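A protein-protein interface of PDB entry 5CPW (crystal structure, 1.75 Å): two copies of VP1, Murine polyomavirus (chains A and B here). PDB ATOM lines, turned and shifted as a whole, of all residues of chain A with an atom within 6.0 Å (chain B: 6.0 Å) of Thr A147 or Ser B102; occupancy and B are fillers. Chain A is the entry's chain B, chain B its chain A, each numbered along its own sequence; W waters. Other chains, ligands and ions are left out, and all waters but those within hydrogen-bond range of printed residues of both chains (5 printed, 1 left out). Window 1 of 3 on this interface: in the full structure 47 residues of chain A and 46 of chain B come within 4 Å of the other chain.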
ATOM      1  N   LEU A 145       3.175  30.307 -16.055  1.00  0.00           N
ATOM      2  CA  LEU A 145       3.299  30.026 -14.624  1.00  0.00           C
ATOM      3  C   LEU A 145       2.016  29.348 -14.175  1.00  0.00           C
ATOM      4  O   LEU A 145       0.915  29.870 -14.404  1.00  0.00           O
ATOM      5  CB  LEU A 145       3.531  31.311 -13.802  1.00  0.00           C
ATOM      6  CG  LEU A 145       3.852  31.148 -12.303  1.00  0.00           C
ATOM      7  CD1 LEU A 145       4.669  32.330 -11.791  1.00  0.00           C
ATOM      8  CD2 LEU A 145       2.580  30.991 -11.464  1.00  0.00           C
ATOM      9  N   VAL A 146       2.157  28.190 -13.532  1.00  0.00           N
ATOM     10  CA  VAL A 146       0.986  27.393 -13.168  1.00  0.00           C
ATOM     11  C   VAL A 146       0.902  27.124 -11.671  1.00  0.00           C
ATOM     12  O   VAL A 146       1.898  27.193 -10.950  1.00  0.00           O
ATOM     13  CB  VAL A 146       0.907  26.050 -13.959  1.00  0.00           C
ATOM     14  CG1 VAL A 146       0.827  26.314 -15.466  1.00  0.00           C
ATOM     15  CG2 VAL A 146       2.081  25.130 -13.640  1.00  0.00           C
ATOM     16  N   THR A 147      -0.308  26.813 -11.219  1.00  0.00           N
ATOM     17  CA  THR A 147      -0.527  26.291  -9.875  1.00  0.00           C
ATOM     18  C   THR A 147       0.198  24.951  -9.644  1.00  0.00           C
ATOM     19  O   THR A 147       0.877  24.757  -8.615  1.00  0.00           O
ATOM     20  CB  THR A 147      -2.046  26.156  -9.601  1.00  0.00           C
ATOM     21  OG1 THR A 147      -2.600  27.456  -9.361  1.00  0.00           O
ATOM     22  CG2 THR A 147      -2.331  25.245  -8.380  1.00  0.00           C
ATOM     23  N   ASP A 148       0.074  24.039 -10.608  1.00  0.00           N
ATOM     24  CA  ASP A 148       0.562  22.674 -10.442  1.00  0.00           C
ATOM     25  C   ASP A 148       1.187  22.194 -11.748  1.00  0.00           C
ATOM     26  O   ASP A 148       0.493  22.026 -12.765  1.00  0.00           O
ATOM     27  CB  ASP A 148      -0.591  21.750 -10.009  1.00  0.00           C
ATOM     28  CG  ASP A 148      -0.115  20.397  -9.485  1.00  0.00           C
ATOM     29  OD1 ASP A 148       1.051  20.012  -9.721  1.00  0.00           O
ATOM     30  OD2 ASP A 148      -0.923  19.707  -8.823  1.00  0.00           O
ATOM     31  N   ALA A 149       2.502  21.982 -11.720  1.00  0.00           N
ATOM     32  CA  ALA A 149       3.238  21.511 -12.896  1.00  0.00           C
ATOM     33  C   ALA A 149       2.841  20.075 -13.258  1.00  0.00           C
ATOM     34  O   ALA A 149       3.222  19.569 -14.322  1.00  0.00           O
ATOM     35  CB  ALA A 149       4.745  21.602 -12.661  1.00  0.00           C
ATOM     36  N   THR A 151      -0.350  19.156 -13.501  1.00  0.00           N
ATOM     37  CA  THR A 151      -1.656  19.241 -14.184  1.00  0.00           C
ATOM     38  C   THR A 151      -1.550  18.669 -15.601  1.00  0.00           C
ATOM     39  O   THR A 151      -0.650  19.029 -16.361  1.00  0.00           O
ATOM     40  CB  THR A 151      -2.194  20.682 -14.243  1.00  0.00           C
ATOM     41  OG1 THR A 151      -2.479  21.140 -12.911  1.00  0.00           O
ATOM     42  CG2 THR A 151      -3.481  20.746 -15.087  1.00  0.00           C
ATOM     43  N   TYR A 153      -2.937  18.875 -18.745  1.00  0.00           N
ATOM     44  CA  TYR A 153      -3.689  19.585 -19.773  1.00  0.00           C
ATOM     45  C   TYR A 153      -3.768  18.731 -21.031  1.00  0.00           C
ATOM     46  O   TYR A 153      -2.858  17.950 -21.312  1.00  0.00           O
ATOM     47  CB  TYR A 153      -3.015  20.916 -20.115  1.00  0.00           C
ATOM     48  CG  TYR A 153      -3.017  21.900 -18.968  1.00  0.00           C
ATOM     49  CD1 TYR A 153      -4.188  22.549 -18.591  1.00  0.00           C
ATOM     50  CD2 TYR A 153      -1.843  22.175 -18.259  1.00  0.00           C
ATOM     51  CE1 TYR A 153      -4.196  23.455 -17.540  1.00  0.00           C
ATOM     52  CE2 TYR A 153      -1.842  23.074 -17.205  1.00  0.00           C
ATOM     53  CZ  TYR A 153      -3.018  23.706 -16.850  1.00  0.00           C
ATOM     54  OH  TYR A 153      -3.006  24.602 -15.809  1.00  0.00           O
ATOM     55  N   ASP A 173       8.115  25.681 -13.212  1.00  0.00           N
ATOM     56  CA  ASP A 173       6.930  26.270 -13.861  1.00  0.00           C
ATOM     57  C   ASP A 173       5.848  26.733 -12.872  1.00  0.00           C
ATOM     58  O   ASP A 173       4.885  27.408 -13.257  1.00  0.00           O
ATOM     59  CB  ASP A 173       6.355  25.300 -14.907  1.00  0.00           C
ATOM     60  CG  ASP A 173       7.277  25.132 -16.119  1.00  0.00           C
ATOM     61  OD1 ASP A 173       7.978  26.103 -16.496  1.00  0.00           O
ATOM     62  OD2 ASP A 173       7.307  24.026 -16.689  1.00  0.00           O
ATOM     63  N   GLN A 174       6.018  26.385 -11.598  1.00  0.00           N
ATOM     64  CA  GLN A 174       5.142  26.892 -10.531  1.00  0.00           C
ATOM     65  C   GLN A 174       5.632  28.229  -9.984  1.00  0.00           C
ATOM     66  O   GLN A 174       4.942  28.877  -9.188  1.00  0.00           O
ATOM     67  CB  GLN A 174       4.982  25.852  -9.418  1.00  0.00           C
ATOM     68  CG  GLN A 174       4.368  24.553  -9.944  1.00  0.00           C
ATOM     69  CD  GLN A 174       4.197  23.462  -8.908  1.00  0.00           C
ATOM     70  OE1 GLN A 174       3.737  22.361  -9.238  1.00  0.00           O
ATOM     71  NE2 GLN A 174       4.563  23.743  -7.654  1.00  0.00           N
ATOM     72  N   VAL A 192      -5.789  31.274 -19.402  1.00  0.00           N
ATOM     73  CA  VAL A 192      -5.359  32.375 -18.525  1.00  0.00           C
ATOM     74  C   VAL A 192      -4.777  31.880 -17.192  1.00  0.00           C
ATOM     75  O   VAL A 192      -4.054  32.613 -16.514  1.00  0.00           O
ATOM     76  CB  VAL A 192      -6.465  33.448 -18.335  1.00  0.00           C
ATOM     77  CG1 VAL A 192      -6.827  34.059 -19.684  1.00  0.00           C
ATOM     78  CG2 VAL A 192      -7.712  32.866 -17.679  1.00  0.00           C
ATOM     79  N   GLU A 193      -5.070  30.638 -16.816  1.00  0.00           N
ATOM     80  CA  GLU A 193      -4.464  30.074 -15.607  1.00  0.00           C
ATOM     81  C   GLU A 193      -3.012  29.626 -15.837  1.00  0.00           C
ATOM     82  O   GLU A 193      -2.318  29.239 -14.890  1.00  0.00           O
ATOM     83  CB  GLU A 193      -5.316  28.934 -15.027  1.00  0.00           C
ATOM     84  CG  GLU A 193      -5.206  27.604 -15.767  1.00  0.00           C
ATOM     85  CD  GLU A 193      -5.883  26.469 -15.012  1.00  0.00           C
ATOM     86  OE1 GLU A 193      -6.966  26.693 -14.436  1.00  0.00           O
ATOM     87  OE2 GLU A 193      -5.337  25.344 -14.992  1.00  0.00           O
ATOM     88  N   ILE A 194      -2.567  29.682 -17.094  1.00  0.00           N
ATOM     89  CA  ILE A 194      -1.196  29.308 -17.479  1.00  0.00           C
ATOM     90  C   ILE A 194      -0.376  30.515 -17.958  1.00  0.00           C
ATOM     91  O   ILE A 194       0.789  30.655 -17.592  1.00  0.00           O
ATOM     92  CB  ILE A 194      -1.180  28.257 -18.616  1.00  0.00           C
ATOM     93  CG1 ILE A 194      -1.910  26.965 -18.207  1.00  0.00           C
ATOM     94  CG2 ILE A 194       0.250  27.962 -19.066  1.00  0.00           C
ATOM     95  CD1 ILE A 194      -2.101  26.004 -19.369  1.00  0.00           C
ATOM     96  N   HIS A 196       0.571  34.493 -18.676  1.00  0.00           N
ATOM     97  CA  HIS A 196       0.524  35.826 -18.073  1.00  0.00           C
ATOM     98  C   HIS A 196       1.306  36.805 -18.931  1.00  0.00           C
ATOM     99  O   HIS A 196       2.256  36.396 -19.607  1.00  0.00           O
ATOM    100  CB  HIS A 196       1.146  35.733 -16.674  1.00  0.00           C
ATOM    101  CG  HIS A 196       0.687  34.517 -15.946  1.00  0.00           C
ATOM    102  ND1 HIS A 196      -0.588  34.410 -15.435  1.00  0.00           N
ATOM    103  CD2 HIS A 196       1.276  33.310 -15.757  1.00  0.00           C
ATOM    104  CE1 HIS A 196      -0.753  33.203 -14.920  1.00  0.00           C
ATOM    105  NE2 HIS A 196       0.362  32.513 -15.108  1.00  0.00           N
ATOM    106  N   GLN B  39       7.097  19.247  -6.235  1.00  0.00           N
ATOM    107  CA  GLN B  39       5.692  19.649  -6.391  1.00  0.00           C
ATOM    108  C   GLN B  39       5.252  20.791  -5.440  1.00  0.00           C
ATOM    109  O   GLN B  39       4.249  21.461  -5.695  1.00  0.00           O
ATOM    110  CB  GLN B  39       4.751  18.429  -6.279  1.00  0.00           C
ATOM    111  CG  GLN B  39       4.632  17.779  -4.893  1.00  0.00           C
ATOM    112  CD  GLN B  39       5.614  16.643  -4.667  1.00  0.00           C
ATOM    113  OE1 GLN B  39       6.797  16.756  -4.982  1.00  0.00           O
ATOM    114  NE2 GLN B  39       5.124  15.531  -4.114  1.00  0.00           N
ATOM    115  N   TYR B  41       7.317  23.399  -4.738  1.00  0.00           N
ATOM    116  CA  TYR B  41       8.078  24.608  -5.062  1.00  0.00           C
ATOM    117  C   TYR B  41       7.146  25.755  -5.498  1.00  0.00           C
ATOM    118  O   TYR B  41       6.298  25.593  -6.375  1.00  0.00           O
ATOM    119  CB  TYR B  41       9.190  24.302  -6.093  1.00  0.00           C
ATOM    120  CG  TYR B  41      10.117  25.465  -6.380  1.00  0.00           C
ATOM    121  CD1 TYR B  41      10.555  26.312  -5.352  1.00  0.00           C
ATOM    122  CD2 TYR B  41      10.576  25.709  -7.675  1.00  0.00           C
ATOM    123  CE1 TYR B  41      11.395  27.383  -5.615  1.00  0.00           C
ATOM    124  CE2 TYR B  41      11.437  26.760  -7.947  1.00  0.00           C
ATOM    125  CZ  TYR B  41      11.838  27.601  -6.912  1.00  0.00           C
ATOM    126  OH  TYR B  41      12.685  28.657  -7.183  1.00  0.00           O
ATOM    127  N   TRP B  43       5.467  27.116  -2.951  1.00  0.00           N
ATOM    128  CA  TRP B  43       4.579  27.007  -1.811  1.00  0.00           C
ATOM    129  C   TRP B  43       5.396  26.653  -0.577  1.00  0.00           C
ATOM    130  O   TRP B  43       6.564  26.289  -0.681  1.00  0.00           O
ATOM    131  CB  TRP B  43       3.564  25.875  -2.014  1.00  0.00           C
ATOM    132  CG  TRP B  43       2.854  25.886  -3.328  1.00  0.00           C
ATOM    133  CD1 TRP B  43       3.349  25.458  -4.530  1.00  0.00           C
ATOM    134  CD2 TRP B  43       1.512  26.325  -3.577  1.00  0.00           C
ATOM    135  NE1 TRP B  43       2.403  25.620  -5.520  1.00  0.00           N
ATOM    136  CE2 TRP B  43       1.264  26.147  -4.965  1.00  0.00           C
ATOM    137  CE3 TRP B  43       0.489  26.844  -2.763  1.00  0.00           C
ATOM    138  CZ2 TRP B  43       0.035  26.474  -5.561  1.00  0.00           C
ATOM    139  CZ3 TRP B  43      -0.725  27.188  -3.356  1.00  0.00           C
ATOM    140  CH2 TRP B  43      -0.947  26.986  -4.740  1.00  0.00           C
ATOM    141  N   GLY B  99       1.845  36.236 -12.281  1.00  0.00           N
ATOM    142  CA  GLY B  99       1.237  34.912 -12.163  1.00  0.00           C
ATOM    143  C   GLY B  99      -0.055  34.826 -11.370  1.00  0.00           C
ATOM    144  O   GLY B  99      -0.507  33.723 -11.056  1.00  0.00           O
ATOM    145  N   SER B 100      -0.675  35.971 -11.060  1.00  0.00           N
ATOM    146  CA  SER B 100      -1.959  35.940 -10.332  1.00  0.00           C
ATOM    147  C   SER B 100      -3.043  35.148 -11.081  1.00  0.00           C
ATOM    148  O   SER B 100      -3.889  34.514 -10.457  1.00  0.00           O
ATOM    149  CB  SER B 100      -2.465  37.344  -9.950  1.00  0.00           C
ATOM    150  OG  SER B 100      -2.755  38.125 -11.095  1.00  0.00           O
ATOM    151  N   GLY B 101      -3.000  35.173 -12.414  1.00  0.00           N
ATOM    152  CA  GLY B 101      -3.909  34.367 -13.229  1.00  0.00           C
ATOM    153  C   GLY B 101      -3.886  32.880 -12.880  1.00  0.00           C
ATOM    154  O   GLY B 101      -4.888  32.186 -13.065  1.00  0.00           O
ATOM    155  N   SER B 102      -2.757  32.386 -12.372  1.00  0.00           N
ATOM    156  CA  SER B 102      -2.637  30.965 -12.014  1.00  0.00           C
ATOM    157  C   SER B 102      -3.559  30.574 -10.855  1.00  0.00           C
ATOM    158  O   SER B 102      -3.884  29.397 -10.678  1.00  0.00           O
ATOM    159  CB  SER B 102      -1.182  30.578 -11.684  1.00  0.00           C
ATOM    160  OG  SER B 102      -0.749  31.115 -10.433  1.00  0.00           O
ATOM    161  N   LEU B 103      -3.981  31.569 -10.074  1.00  0.00           N
ATOM    162  CA  LEU B 103      -4.871  31.339  -8.935  1.00  0.00           C
ATOM    163  C   LEU B 103      -6.312  31.054  -9.391  1.00  0.00           C
ATOM    164  O   LEU B 103      -7.159  30.684  -8.581  1.00  0.00           O
ATOM    165  CB  LEU B 103      -4.823  32.533  -7.968  1.00  0.00           C
ATOM    166  CG  LEU B 103      -3.416  32.879  -7.446  1.00  0.00           C
ATOM    167  CD1 LEU B 103      -3.483  34.142  -6.598  1.00  0.00           C
ATOM    168  CD2 LEU B 103      -2.816  31.731  -6.649  1.00  0.00           C
ATOM    169  N   LEU B 104      -6.565  31.221 -10.691  1.00  0.00           N
ATOM    170  CA  LEU B 104      -7.851  30.872 -11.311  1.00  0.00           C
ATOM    171  C   LEU B 104      -7.990  29.357 -11.546  1.00  0.00           C
ATOM    172  O   LEU B 104      -9.026  28.894 -12.012  1.00  0.00           O
ATOM    173  CB  LEU B 104      -8.045  31.626 -12.627  1.00  0.00           C
ATOM    174  CG  LEU B 104      -8.065  33.164 -12.512  1.00  0.00           C
ATOM    175  CD1 LEU B 104      -7.899  33.786 -13.886  1.00  0.00           C
ATOM    176  CD2 LEU B 104      -9.354  33.643 -11.851  1.00  0.00           C
ATOM    177  N   ASP B 105      -6.943  28.602 -11.222  1.00  0.00           N
ATOM    178  CA  ASP B 105      -7.043  27.141 -11.223  1.00  0.00           C
ATOM    179  C   ASP B 105      -7.857  26.693 -10.003  1.00  0.00           C
ATOM    180  O   ASP B 105      -7.341  26.624  -8.887  1.00  0.00           O
ATOM    181  CB  ASP B 105      -5.642  26.492 -11.250  1.00  0.00           C
ATOM    182  CG  ASP B 105      -5.676  24.982 -10.991  1.00  0.00           C
ATOM    183  OD1 ASP B 105      -6.772  24.396 -10.850  1.00  0.00           O
ATOM    184  OD2 ASP B 105      -4.589  24.373 -10.926  1.00  0.00           O
ATOM    185  N   ARG B 257      -3.384  27.741   0.198  1.00  0.00           N
ATOM    186  CA  ARG B 257      -4.337  26.718  -0.232  1.00  0.00           C
ATOM    187  C   ARG B 257      -4.533  25.765   0.945  1.00  0.00           C
ATOM    188  O   ARG B 257      -3.673  25.676   1.837  1.00  0.00           O
ATOM    189  CB  ARG B 257      -3.885  25.973  -1.496  1.00  0.00           C
ATOM    190  CG  ARG B 257      -2.716  25.019  -1.297  1.00  0.00           C
ATOM    191  CD  ARG B 257      -2.411  24.246  -2.572  1.00  0.00           C
ATOM    192  NE  ARG B 257      -1.243  23.391  -2.396  1.00  0.00           N
ATOM    193  CZ  ARG B 257      -1.283  22.184  -1.844  1.00  0.00           C
ATOM    194  NH1 ARG B 257      -2.436  21.685  -1.422  1.00  0.00           N
ATOM    195  NH2 ARG B 257      -0.172  21.473  -1.717  1.00  0.00           N
ATOM    196  N   ARG B 268       1.199  30.299  -0.421  1.00  0.00           N
ATOM    197  CA  ARG B 268       1.491  30.509  -1.853  1.00  0.00           C
ATOM    198  C   ARG B 268       2.184  31.850  -2.032  1.00  0.00           C
ATOM    199  O   ARG B 268       1.707  32.873  -1.529  1.00  0.00           O
ATOM    200  CB  ARG B 268       0.206  30.488  -2.706  1.00  0.00           C
ATOM    201  CG  ARG B 268       0.402  30.734  -4.224  1.00  0.00           C
ATOM    202  CD  ARG B 268       1.444  29.801  -4.843  1.00  0.00           C
ATOM    203  NE  ARG B 268       1.293  29.586  -6.293  1.00  0.00           N
ATOM    204  CZ  ARG B 268       2.304  29.335  -7.125  1.00  0.00           C
ATOM    205  NH1 ARG B 268       3.564  29.328  -6.674  1.00  0.00           N
ATOM    206  NH2 ARG B 268       2.063  29.099  -8.416  1.00  0.00           N
ATOM    207  N   LEU B 270       4.354  34.351  -5.154  1.00  0.00           N
ATOM    208  CA  LEU B 270       4.540  34.592  -6.586  1.00  0.00           C
ATOM    209  C   LEU B 270       5.841  35.357  -6.836  1.00  0.00           C
ATOM    210  O   LEU B 270       6.289  36.112  -5.967  1.00  0.00           O
ATOM    211  CB  LEU B 270       3.348  35.363  -7.177  1.00  0.00           C
ATOM    212  CG  LEU B 270       2.016  34.609  -7.310  1.00  0.00           C
ATOM    213  CD1 LEU B 270       0.933  35.550  -7.844  1.00  0.00           C
ATOM    214  CD2 LEU B 270       2.153  33.374  -8.201  1.00  0.00           C
HETATM  215  O   HOH W   1      -4.958  27.415  -7.664  1.00  0.00           O
HETATM  216  O   HOH W   2      -1.601  36.792 -14.399  1.00  0.00           O
HETATM  217  O   HOH W   3      -8.906  28.454 -15.199  1.00  0.00           O
HETATM  218  O   HOH W   4      -0.837  29.403  -8.346  1.00  0.00           O
HETATM  219  O   HOH W   5      -2.160  24.012 -12.631  1.00  0.00           O
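No position is printed for both chains.
Of the 19 pairs that touch across the chains among the printed residues, none has its exchanged pair printed and touching as well.
Ser B102 touches just these residues of chain A: Leu A145 (3.5 Å), Thr A147 (2.7 Å), Glu A193 (3.4 Å) and His A196 (3.3 Å).
Of the printed residues of chain A, Arg B268 touches Leu A145 (3.6 Å), Val A146 (3.2 Å) and Gln A174 (2.9 Å).
Printed residues of chain B within 4 Å of Val A192: Gly B101 and Leu B104.
Leu B103 touches none of the printed residues of chain A.
The nearest residue of chain A that does not touch Ser B102 is Val A146 (4.03 Å).
Among the printed residues, pairs that only touch across the chains: Glu A193 with Asp B105, Glu A193 with Gly B101, His A196 with Ser B102, Glu A193 with Ser B102, Thr A147 with Asp B105, Leu A145 with Ser B102, Thr A147 with Trp B43, Gln A174 with Trp B43, Val A192 with Gly B101, Leu A145 with Arg B268, His A196 with Gly B101, His A196 with Gly B99, Glu A193 with Leu B104 and Val A192 with Leu B104.
OG of Ser B102 sits at hydrogen-bond distance from O of Gly B99 (2.7 Å).
N of Leu A145 lies within hydrogen-bond range of O of Ile A194 (2.9 Å).
The backbone NH (N) of Val A146 is in hydrogen-bond range of the backbone carbonyl oxygen (O) of Asp A173, at 2.9 Å.
OE1 of Gln A174 is in hydrogen-bond range of N of Ala A149 (2.8 Å).
OH of Tyr A153 sits at hydrogen-bond distance from OE2 of Glu A193, 2.6 Å away.
O of Ile A194 sits at hydrogen-bond distance from NE2 of His A196.
Hydrophobic or aromatic side chains of chain B that line the printed part of chain A: Trp B43 and Leu B104.
Among the printed residues, 19 pairs touch across the chains.
Water W4 lies within hydrogen-bond range of the side-chain hydroxyl of Ser B102 (2.7 Å), the side-chain hydroxyl of Thr A147 (2.8 Å) and the guanidinium group of Arg B268 (2.9 Å).
Water W3 lies within hydrogen-bond range of the side-chain carboxylate of Glu A193 and the backbone carbonyl oxygen of Leu B104.
Water W2 bridges ND1 of His A196 and N of Gly B101.
Water W1 bridges the backbone carbonyl oxygen (O) of Asp B105 (2.8 Å) and the side-chain hydroxyl (OG1) of Thr A147 (2.9 Å).
Water W5 lies within hydrogen-bond range of OG1 of Thr A151, OD2 of Asp B105, N of Asp A148 and OH of Tyr A153.
The backbone carbonyl oxygen of Gln B39 is in hydrogen-bond range of the side-chain amide nitrogen of Gln A174 (3.0 Å).
O of Tyr B41 lies within hydrogen-bond range of NE2 of Gln A174 (2.8 Å).
The side-chain hydroxyl (OG1) of Thr A147 is in hydrogen-bond range of the backbone carbonyl oxygen (O) of Ser B102.
The guanidinium group (NH2) of Arg B268 is in hydrogen-bond range of the backbone carbonyl oxygen (O) of Val A146 (3.2 Å).
The guanidinium group of Arg B268 sits at hydrogen-bond distance from the backbone carbonyl oxygen of Gln A174, 2.9 Å away.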
